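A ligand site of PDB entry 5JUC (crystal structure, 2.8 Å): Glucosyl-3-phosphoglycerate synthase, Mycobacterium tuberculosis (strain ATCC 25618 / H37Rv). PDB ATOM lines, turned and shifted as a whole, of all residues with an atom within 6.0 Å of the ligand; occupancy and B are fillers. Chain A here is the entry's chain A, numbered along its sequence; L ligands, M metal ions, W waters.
The side-chain carboxylate (OE2) of Glu 58 is in hydrogen-bond range of an oxygen (O3) of the ligand (2.8 Å).
The side-chain hydroxyl (OH) of Tyr 233 lies within hydrogen-bond range of an oxygen (O8) of the ligand.
N of Leu 56 is in hydrogen-bond range of O3 of the ligand (2.8 Å).
N2 of the ligand sits at hydrogen-bond distance from OG of Ser 85, 3.0 Å away.
The backbone NH of Ser 139 sits at hydrogen-bond distance from an oxygen (O5) of the ligand, at 3.2 Å.
O5 of the ligand is in hydrogen-bond range of OG of Ser 139 (3.1 Å).
NE of Arg 265 is in salt-bridge range of O12 of the ligand, at 3.1 Å.
An oxygen (O5) of the ligand is in hydrogen-bond range of the backbone carbonyl oxygen of Pro 54, 3.3 Å away.
N of Ala 55 is in hydrogen-bond range of O1 of the ligand (3.3 Å).
The backbone NH (N) of Lys 118 sits at hydrogen-bond distance from an oxygen (O2) of the ligand (3.4 Å).
N of Ser 85 lies within hydrogen-bond range of O of Ala 55 (2.8 Å).
The backbone carbonyl oxygen of Ser 85 sits at hydrogen-bond distance from the guanidinium group of Arg 105 (3.2 Å).
The side-chain hydroxyl (OG) of Ser 139 sits at hydrogen-bond distance from the backbone carbonyl oxygen (O) of Pro 54 (2.6 Å).
The backbone carbonyl oxygen (O) of Leu 83 lies within hydrogen-bond range of the backbone NH (N) of Ala 55, 3.1 Å away.
The side-chain amino group (NZ) of Lys 118 is in salt-bridge range of the side-chain carboxylate (OD1) of Asp 138 (3.0 Å).
O of Gly 117 lies close to O2 of the ligand (3.4 Å).
O9 of the ligand sits close to OD1 of Asp 140 (3.1 Å).
Residues that only touch the ligand: Asp 138 and Arg 263.
Hydrophobic or aromatic side chains that line the ligand: Pro 54, Leu 56 and Tyr 233.
Of the 22 residues printed, 13 come within 4 Å of the ligand.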
ATOM      1  N   PRO A  54      23.098  17.661 -22.635  1.00  0.00           N
ATOM      2  CA  PRO A  54      24.261  18.511 -22.950  1.00  0.00           C
ATOM      3  C   PRO A  54      24.531  19.451 -21.793  1.00  0.00           C
ATOM      4  O   PRO A  54      23.607  20.016 -21.209  1.00  0.00           O
ATOM      5  CB  PRO A  54      23.819  19.268 -24.212  1.00  0.00           C
ATOM      6  CG  PRO A  54      22.326  19.406 -24.012  1.00  0.00           C
ATOM      7  CD  PRO A  54      21.900  18.090 -23.385  1.00  0.00           C
ATOM      8  N   ALA A  55      25.812  19.620 -21.466  1.00  0.00           N
ATOM      9  CA  ALA A  55      26.180  20.357 -20.271  1.00  0.00           C
ATOM     10  C   ALA A  55      27.391  21.240 -20.548  1.00  0.00           C
ATOM     11  O   ALA A  55      28.470  20.737 -20.858  1.00  0.00           O
ATOM     12  CB  ALA A  55      26.487  19.401 -19.108  1.00  0.00           C
ATOM     13  N   LEU A  56      27.201  22.551 -20.411  1.00  0.00           N
ATOM     14  CA  LEU A  56      28.305  23.509 -20.371  1.00  0.00           C
ATOM     15  C   LEU A  56      28.165  24.295 -19.073  1.00  0.00           C
ATOM     16  O   LEU A  56      27.344  25.205 -18.973  1.00  0.00           O
ATOM     17  CB  LEU A  56      28.300  24.439 -21.582  1.00  0.00           C
ATOM     18  CG  LEU A  56      29.361  25.553 -21.539  1.00  0.00           C
ATOM     19  CD1 LEU A  56      30.761  24.964 -21.350  1.00  0.00           C
ATOM     20  CD2 LEU A  56      29.304  26.399 -22.791  1.00  0.00           C
ATOM     21  N   ASN A  57      28.988  23.928 -18.072  1.00  0.00           N
ATOM     22  CA  ASN A  57      29.075  24.616 -16.785  1.00  0.00           C
ATOM     23  C   ASN A  57      27.713  24.671 -16.077  1.00  0.00           C
ATOM     24  O   ASN A  57      27.069  25.713 -15.967  1.00  0.00           O
ATOM     25  CB  ASN A  57      29.627  26.043 -16.965  1.00  0.00           C
ATOM     26  CG  ASN A  57      31.025  26.054 -17.560  1.00  0.00           C
ATOM     27  OD1 ASN A  57      31.859  25.210 -17.223  1.00  0.00           O
ATOM     28  ND2 ASN A  57      31.280  27.004 -18.464  1.00  0.00           N
ATOM     29  N   GLU A  58      27.303  23.496 -15.583  1.00  0.00           N
ATOM     30  CA  GLU A  58      25.995  23.345 -14.941  1.00  0.00           C
ATOM     31  C   GLU A  58      26.101  22.601 -13.600  1.00  0.00           C
ATOM     32  O   GLU A  58      25.162  21.924 -13.187  1.00  0.00           O
ATOM     33  CB  GLU A  58      25.018  22.627 -15.873  1.00  0.00           C
ATOM     34  CG  GLU A  58      24.957  23.185 -17.282  1.00  0.00           C
ATOM     35  CD  GLU A  58      24.345  24.582 -17.357  1.00  0.00           C
ATOM     36  OE1 GLU A  58      23.767  25.048 -16.351  1.00  0.00           O
ATOM     37  OE2 GLU A  58      24.435  25.212 -18.435  1.00  0.00           O
ATOM     38  N   LEU A  83      26.849  14.831 -22.181  1.00  0.00           N
ATOM     39  CA  LEU A  83      27.844  15.278 -23.142  1.00  0.00           C
ATOM     40  C   LEU A  83      28.442  16.584 -22.641  1.00  0.00           C
ATOM     41  O   LEU A  83      27.801  17.638 -22.715  1.00  0.00           O
ATOM     42  CB  LEU A  83      27.260  15.456 -24.545  1.00  0.00           C
ATOM     43  CG  LEU A  83      28.444  15.464 -25.518  1.00  0.00           C
ATOM     44  CD1 LEU A  83      28.365  14.282 -26.452  1.00  0.00           C
ATOM     45  CD2 LEU A  83      28.517  16.775 -26.257  1.00  0.00           C
ATOM     46  N   SER A  85      30.148  19.701 -22.812  1.00  0.00           N
ATOM     47  CA  SER A  85      30.485  20.665 -23.855  1.00  0.00           C
ATOM     48  C   SER A  85      31.603  21.627 -23.451  1.00  0.00           C
ATOM     49  O   SER A  85      31.560  22.816 -23.782  1.00  0.00           O
ATOM     50  CB  SER A  85      29.207  21.432 -24.218  1.00  0.00           C
ATOM     51  OG  SER A  85      29.371  22.183 -25.401  1.00  0.00           O
ATOM     52  N   ARG A 105      33.054  16.267 -25.936  1.00  0.00           N
ATOM     53  CA  ARG A 105      32.905  16.440 -27.382  1.00  0.00           C
ATOM     54  C   ARG A 105      34.012  15.708 -28.121  1.00  0.00           C
ATOM     55  O   ARG A 105      33.755  15.033 -29.126  1.00  0.00           O
ATOM     56  CB  ARG A 105      32.899  17.928 -27.728  1.00  0.00           C
ATOM     57  CG  ARG A 105      31.676  18.679 -27.181  1.00  0.00           C
ATOM     58  CD  ARG A 105      31.832  20.193 -27.227  1.00  0.00           C
ATOM     59  NE  ARG A 105      33.089  20.627 -26.639  1.00  0.00           N
ATOM     60  CZ  ARG A 105      33.436  21.899 -26.463  1.00  0.00           C
ATOM     61  NH1 ARG A 105      32.631  22.880 -26.819  1.00  0.00           N
ATOM     62  NH2 ARG A 105      34.619  22.188 -25.927  1.00  0.00           N
ATOM     63  N   PRO A 116      32.597  25.310 -31.158  1.00  0.00           N
ATOM     64  CA  PRO A 116      31.787  25.749 -30.020  1.00  0.00           C
ATOM     65  C   PRO A 116      30.294  25.621 -30.295  1.00  0.00           C
ATOM     66  O   PRO A 116      29.848  25.387 -31.422  1.00  0.00           O
ATOM     67  CB  PRO A 116      32.194  27.212 -29.829  1.00  0.00           C
ATOM     68  CG  PRO A 116      32.799  27.636 -31.105  1.00  0.00           C
ATOM     69  CD  PRO A 116      33.371  26.414 -31.760  1.00  0.00           C
ATOM     70  N   GLY A 117      29.515  25.794 -29.235  1.00  0.00           N
ATOM     71  CA  GLY A 117      28.085  25.952 -29.338  1.00  0.00           C
ATOM     72  C   GLY A 117      27.311  24.683 -29.014  1.00  0.00           C
ATOM     73  O   GLY A 117      27.852  23.577 -28.990  1.00  0.00           O
ATOM     74  N   LYS A 118      26.011  24.871 -28.800  1.00  0.00           N
ATOM     75  CA  LYS A 118      25.159  23.775 -28.376  1.00  0.00           C
ATOM     76  C   LYS A 118      24.934  22.786 -29.503  1.00  0.00           C
ATOM     77  O   LYS A 118      25.096  21.568 -29.311  1.00  0.00           O
ATOM     78  CB  LYS A 118      23.829  24.333 -27.877  1.00  0.00           C
ATOM     79  CG  LYS A 118      22.941  23.312 -27.174  1.00  0.00           C
ATOM     80  CD  LYS A 118      21.576  23.914 -26.866  1.00  0.00           C
ATOM     81  CE  LYS A 118      20.697  22.943 -26.099  1.00  0.00           C
ATOM     82  NZ  LYS A 118      19.409  23.571 -25.720  1.00  0.00           N
ATOM     83  N   ALA A 121      27.371  20.052 -29.703  1.00  0.00           N
ATOM     84  CA  ALA A 121      27.312  19.018 -28.672  1.00  0.00           C
ATOM     85  C   ALA A 121      26.213  18.002 -28.955  1.00  0.00           C
ATOM     86  O   ALA A 121      26.428  16.795 -28.803  1.00  0.00           O
ATOM     87  CB  ALA A 121      27.092  19.687 -27.310  1.00  0.00           C
ATOM     88  N   ILE A 137      17.478  16.389 -22.926  1.00  0.00           N
ATOM     89  CA  ILE A 137      17.046  17.154 -21.755  1.00  0.00           C
ATOM     90  C   ILE A 137      18.130  18.161 -21.409  1.00  0.00           C
ATOM     91  O   ILE A 137      19.290  17.780 -21.217  1.00  0.00           O
ATOM     92  CB  ILE A 137      16.760  16.266 -20.527  1.00  0.00           C
ATOM     93  CG1 ILE A 137      16.024  14.981 -20.888  1.00  0.00           C
ATOM     94  CG2 ILE A 137      15.966  17.067 -19.475  1.00  0.00           C
ATOM     95  CD1 ILE A 137      14.537  15.145 -21.179  1.00  0.00           C
ATOM     96  N   ASP A 138      17.750  19.438 -21.309  1.00  0.00           N
ATOM     97  CA  ASP A 138      18.708  20.443 -20.890  1.00  0.00           C
ATOM     98  C   ASP A 138      19.155  20.178 -19.452  1.00  0.00           C
ATOM     99  O   ASP A 138      18.351  19.816 -18.583  1.00  0.00           O
ATOM    100  CB  ASP A 138      18.099  21.843 -21.006  1.00  0.00           C
ATOM    101  CG  ASP A 138      18.119  22.383 -22.439  1.00  0.00           C
ATOM    102  OD1 ASP A 138      18.945  21.910 -23.256  1.00  0.00           O
ATOM    103  OD2 ASP A 138      17.327  23.300 -22.744  1.00  0.00           O
ATOM    104  N   SER A 139      20.453  20.353 -19.216  1.00  0.00           N
ATOM    105  CA  SER A 139      21.059  20.077 -17.918  1.00  0.00           C
ATOM    106  C   SER A 139      20.987  21.270 -16.974  1.00  0.00           C
ATOM    107  O   SER A 139      21.559  21.219 -15.876  1.00  0.00           O
ATOM    108  CB  SER A 139      22.515  19.638 -18.114  1.00  0.00           C
ATOM    109  OG  SER A 139      23.303  20.667 -18.673  1.00  0.00           O
ATOM    110  N   ASP A 140      20.289  22.341 -17.358  1.00  0.00           N
ATOM    111  CA  ASP A 140      20.144  23.532 -16.530  1.00  0.00           C
ATOM    112  C   ASP A 140      18.737  23.690 -15.963  1.00  0.00           C
ATOM    113  O   ASP A 140      18.371  24.768 -15.496  1.00  0.00           O
ATOM    114  CB  ASP A 140      20.548  24.783 -17.320  1.00  0.00           C
ATOM    115  CG  ASP A 140      19.602  25.094 -18.473  1.00  0.00           C
ATOM    116  OD1 ASP A 140      19.525  26.271 -18.896  1.00  0.00           O
ATOM    117  OD2 ASP A 140      18.935  24.168 -18.977  1.00  0.00           O
ATOM    118  N   TYR A 233      22.915  27.951 -30.653  1.00  0.00           N
ATOM    119  CA  TYR A 233      21.496  27.976 -30.298  1.00  0.00           C
ATOM    120  C   TYR A 233      20.569  27.867 -31.465  1.00  0.00           C
ATOM    121  O   TYR A 233      19.385  28.045 -31.201  1.00  0.00           O
ATOM    122  CB  TYR A 233      21.188  29.251 -29.514  1.00  0.00           C
ATOM    123  CG  TYR A 233      21.967  29.357 -28.225  1.00  0.00           C
ATOM    124  CD1 TYR A 233      21.765  28.441 -27.211  1.00  0.00           C
ATOM    125  CD2 TYR A 233      22.901  30.359 -28.040  1.00  0.00           C
ATOM    126  CE1 TYR A 233      22.480  28.524 -26.034  1.00  0.00           C
ATOM    127  CE2 TYR A 233      23.617  30.451 -26.874  1.00  0.00           C
ATOM    128  CZ  TYR A 233      23.406  29.533 -25.871  1.00  0.00           C
ATOM    129  OH  TYR A 233      24.121  29.626 -24.695  1.00  0.00           O
ATOM    130  N   HIS A 262      14.480  27.651 -15.197  1.00  0.00           N
ATOM    131  CA  HIS A 262      15.892  27.507 -15.543  1.00  0.00           C
ATOM    132  C   HIS A 262      16.528  28.856 -15.269  1.00  0.00           C
ATOM    133  O   HIS A 262      15.842  29.815 -14.925  1.00  0.00           O
ATOM    134  CB  HIS A 262      16.082  27.068 -17.003  1.00  0.00           C
ATOM    135  CG  HIS A 262      15.676  28.096 -18.012  1.00  0.00           C
ATOM    136  ND1 HIS A 262      16.290  28.191 -19.246  1.00  0.00           N
ATOM    137  CD2 HIS A 262      14.733  29.062 -17.989  1.00  0.00           C
ATOM    138  CE1 HIS A 262      15.739  29.176 -19.932  1.00  0.00           C
ATOM    139  NE2 HIS A 262      14.794  29.724 -19.204  1.00  0.00           N
ATOM    140  N   ARG A 263      17.846  28.922 -15.400  1.00  0.00           N
ATOM    141  CA  ARG A 263      18.500  30.225 -15.422  1.00  0.00           C
ATOM    142  C   ARG A 263      17.689  31.144 -16.317  1.00  0.00           C
ATOM    143  O   ARG A 263      17.294  30.758 -17.417  1.00  0.00           O
ATOM    144  CB  ARG A 263      19.926  30.113 -15.945  1.00  0.00           C
ATOM    145  CG  ARG A 263      20.503  31.455 -16.404  1.00  0.00           C
ATOM    146  N   ASN A 264      17.482  32.363 -15.862  1.00  0.00           N
ATOM    147  CA  ASN A 264      16.966  33.422 -16.710  1.00  0.00           C
ATOM    148  C   ASN A 264      18.092  34.403 -16.977  1.00  0.00           C
ATOM    149  O   ASN A 264      18.519  35.122 -16.069  1.00  0.00           O
ATOM    150  CB  ASN A 264      15.752  34.085 -16.068  1.00  0.00           C
ATOM    151  CG  ASN A 264      14.451  33.303 -16.299  1.00  0.00           C
ATOM    152  OD1 ASN A 264      14.443  32.070 -16.279  1.00  0.00           O
ATOM    153  ND2 ASN A 264      13.351  34.008 -16.529  1.00  0.00           N
ATOM    154  N   ARG A 265      18.544  34.446 -18.223  1.00  0.00           N
ATOM    155  CA  ARG A 265      19.834  34.997 -18.584  1.00  0.00           C
ATOM    156  C   ARG A 265      19.740  36.490 -18.805  1.00  0.00           C
ATOM    157  O   ARG A 265      18.657  37.089 -18.794  1.00  0.00           O
ATOM    158  CB  ARG A 265      20.348  34.314 -19.845  1.00  0.00           C
ATOM    159  CG  ARG A 265      19.977  32.847 -19.982  1.00  0.00           C
ATOM    160  CD  ARG A 265      20.746  32.196 -21.130  1.00  0.00           C
ATOM    161  NE  ARG A 265      22.117  31.884 -20.732  1.00  0.00           N
ATOM    162  CZ  ARG A 265      23.193  32.042 -21.492  1.00  0.00           C
ATOM    163  NH1 ARG A 265      23.096  32.549 -22.723  1.00  0.00           N
ATOM    164  NH2 ARG A 265      24.376  31.715 -21.012  1.00  0.00           N
ATOM    165  N   MET A 273      21.736  34.702 -28.836  1.00  0.00           N
ATOM    166  CA  MET A 273      20.871  33.560 -29.116  1.00  0.00           C
ATOM    167  C   MET A 273      19.841  33.910 -30.178  1.00  0.00           C
ATOM    168  O   MET A 273      19.615  33.141 -31.126  1.00  0.00           O
ATOM    169  CB  MET A 273      20.183  33.104 -27.819  1.00  0.00           C
ATOM    170  CG  MET A 273      19.274  31.870 -27.986  1.00  0.00           C
ATOM    171  SD  MET A 273      18.202  31.528 -26.568  1.00  0.00           S
ATOM    172  CE  MET A 273      19.342  31.767 -25.186  1.00  0.00           C
HETATM  173  N1  LIG L   1      24.931  24.115 -23.738  1.00  0.00           N
HETATM  174  C1  LIG L   1      25.932  23.236 -24.086  1.00  0.00           C
HETATM  175  N2  LIG L   1      26.902  23.755 -24.918  1.00  0.00           N
HETATM  176  C2  LIG L   1      26.975  25.047 -25.391  1.00  0.00           C
HETATM  177  C3  LIG L   1      25.899  25.897 -24.993  1.00  0.00           C
HETATM  178  C4  LIG L   1      24.933  25.413 -24.196  1.00  0.00           C
HETATM  179  O1  LIG L   1      25.981  22.079 -23.678  1.00  0.00           O
HETATM  180  O2  LIG L   1      27.946  25.385 -26.083  1.00  0.00           O
HETATM  181  C5  LIG L   1      23.830  23.604 -22.905  1.00  0.00           C
HETATM  182  C6  LIG L   1      23.785  24.217 -21.503  1.00  0.00           C
HETATM  183  O3  LIG L   1      24.594  23.493 -20.589  1.00  0.00           O
HETATM  184  C7  LIG L   1      22.297  24.072 -21.157  1.00  0.00           C
HETATM  185  C8  LIG L   1      21.595  24.185 -22.506  1.00  0.00           C
HETATM  186  O4  LIG L   1      22.608  23.965 -23.514  1.00  0.00           O
HETATM  187  O5  LIG L   1      22.036  22.812 -20.559  1.00  0.00           O
HETATM  188  C9  LIG L   1      20.902  25.496 -22.776  1.00  0.00           C
HETATM  189  O6  LIG L   1      21.864  26.568 -22.651  1.00  0.00           O
HETATM  190  P1  LIG L   1      21.570  28.025 -22.067  1.00  0.00           P
HETATM  191  O7  LIG L   1      20.303  28.572 -22.606  1.00  0.00           O
HETATM  192  O8  LIG L   1      22.748  28.917 -22.428  1.00  0.00           O
HETATM  193  O9  LIG L   1      21.515  27.958 -20.477  1.00  0.00           O
HETATM  194  P2  LIG L   1      22.550  28.360 -19.330  1.00  0.00           P
HETATM  195  O10 LIG L   1      23.866  28.778 -20.014  1.00  0.00           O
HETATM  196  O11 LIG L   1      22.753  27.248 -18.362  1.00  0.00           O
HETATM  197  O12 LIG L   1      21.944  29.570 -18.635  1.00  0.00           O
HETATM  198 MN    MN M   1      17.900  26.873 -20.156  1.00  0.00          MN
HETATM  199  O   HOH W   1      17.593  29.436 -22.809  1.00  0.00           O
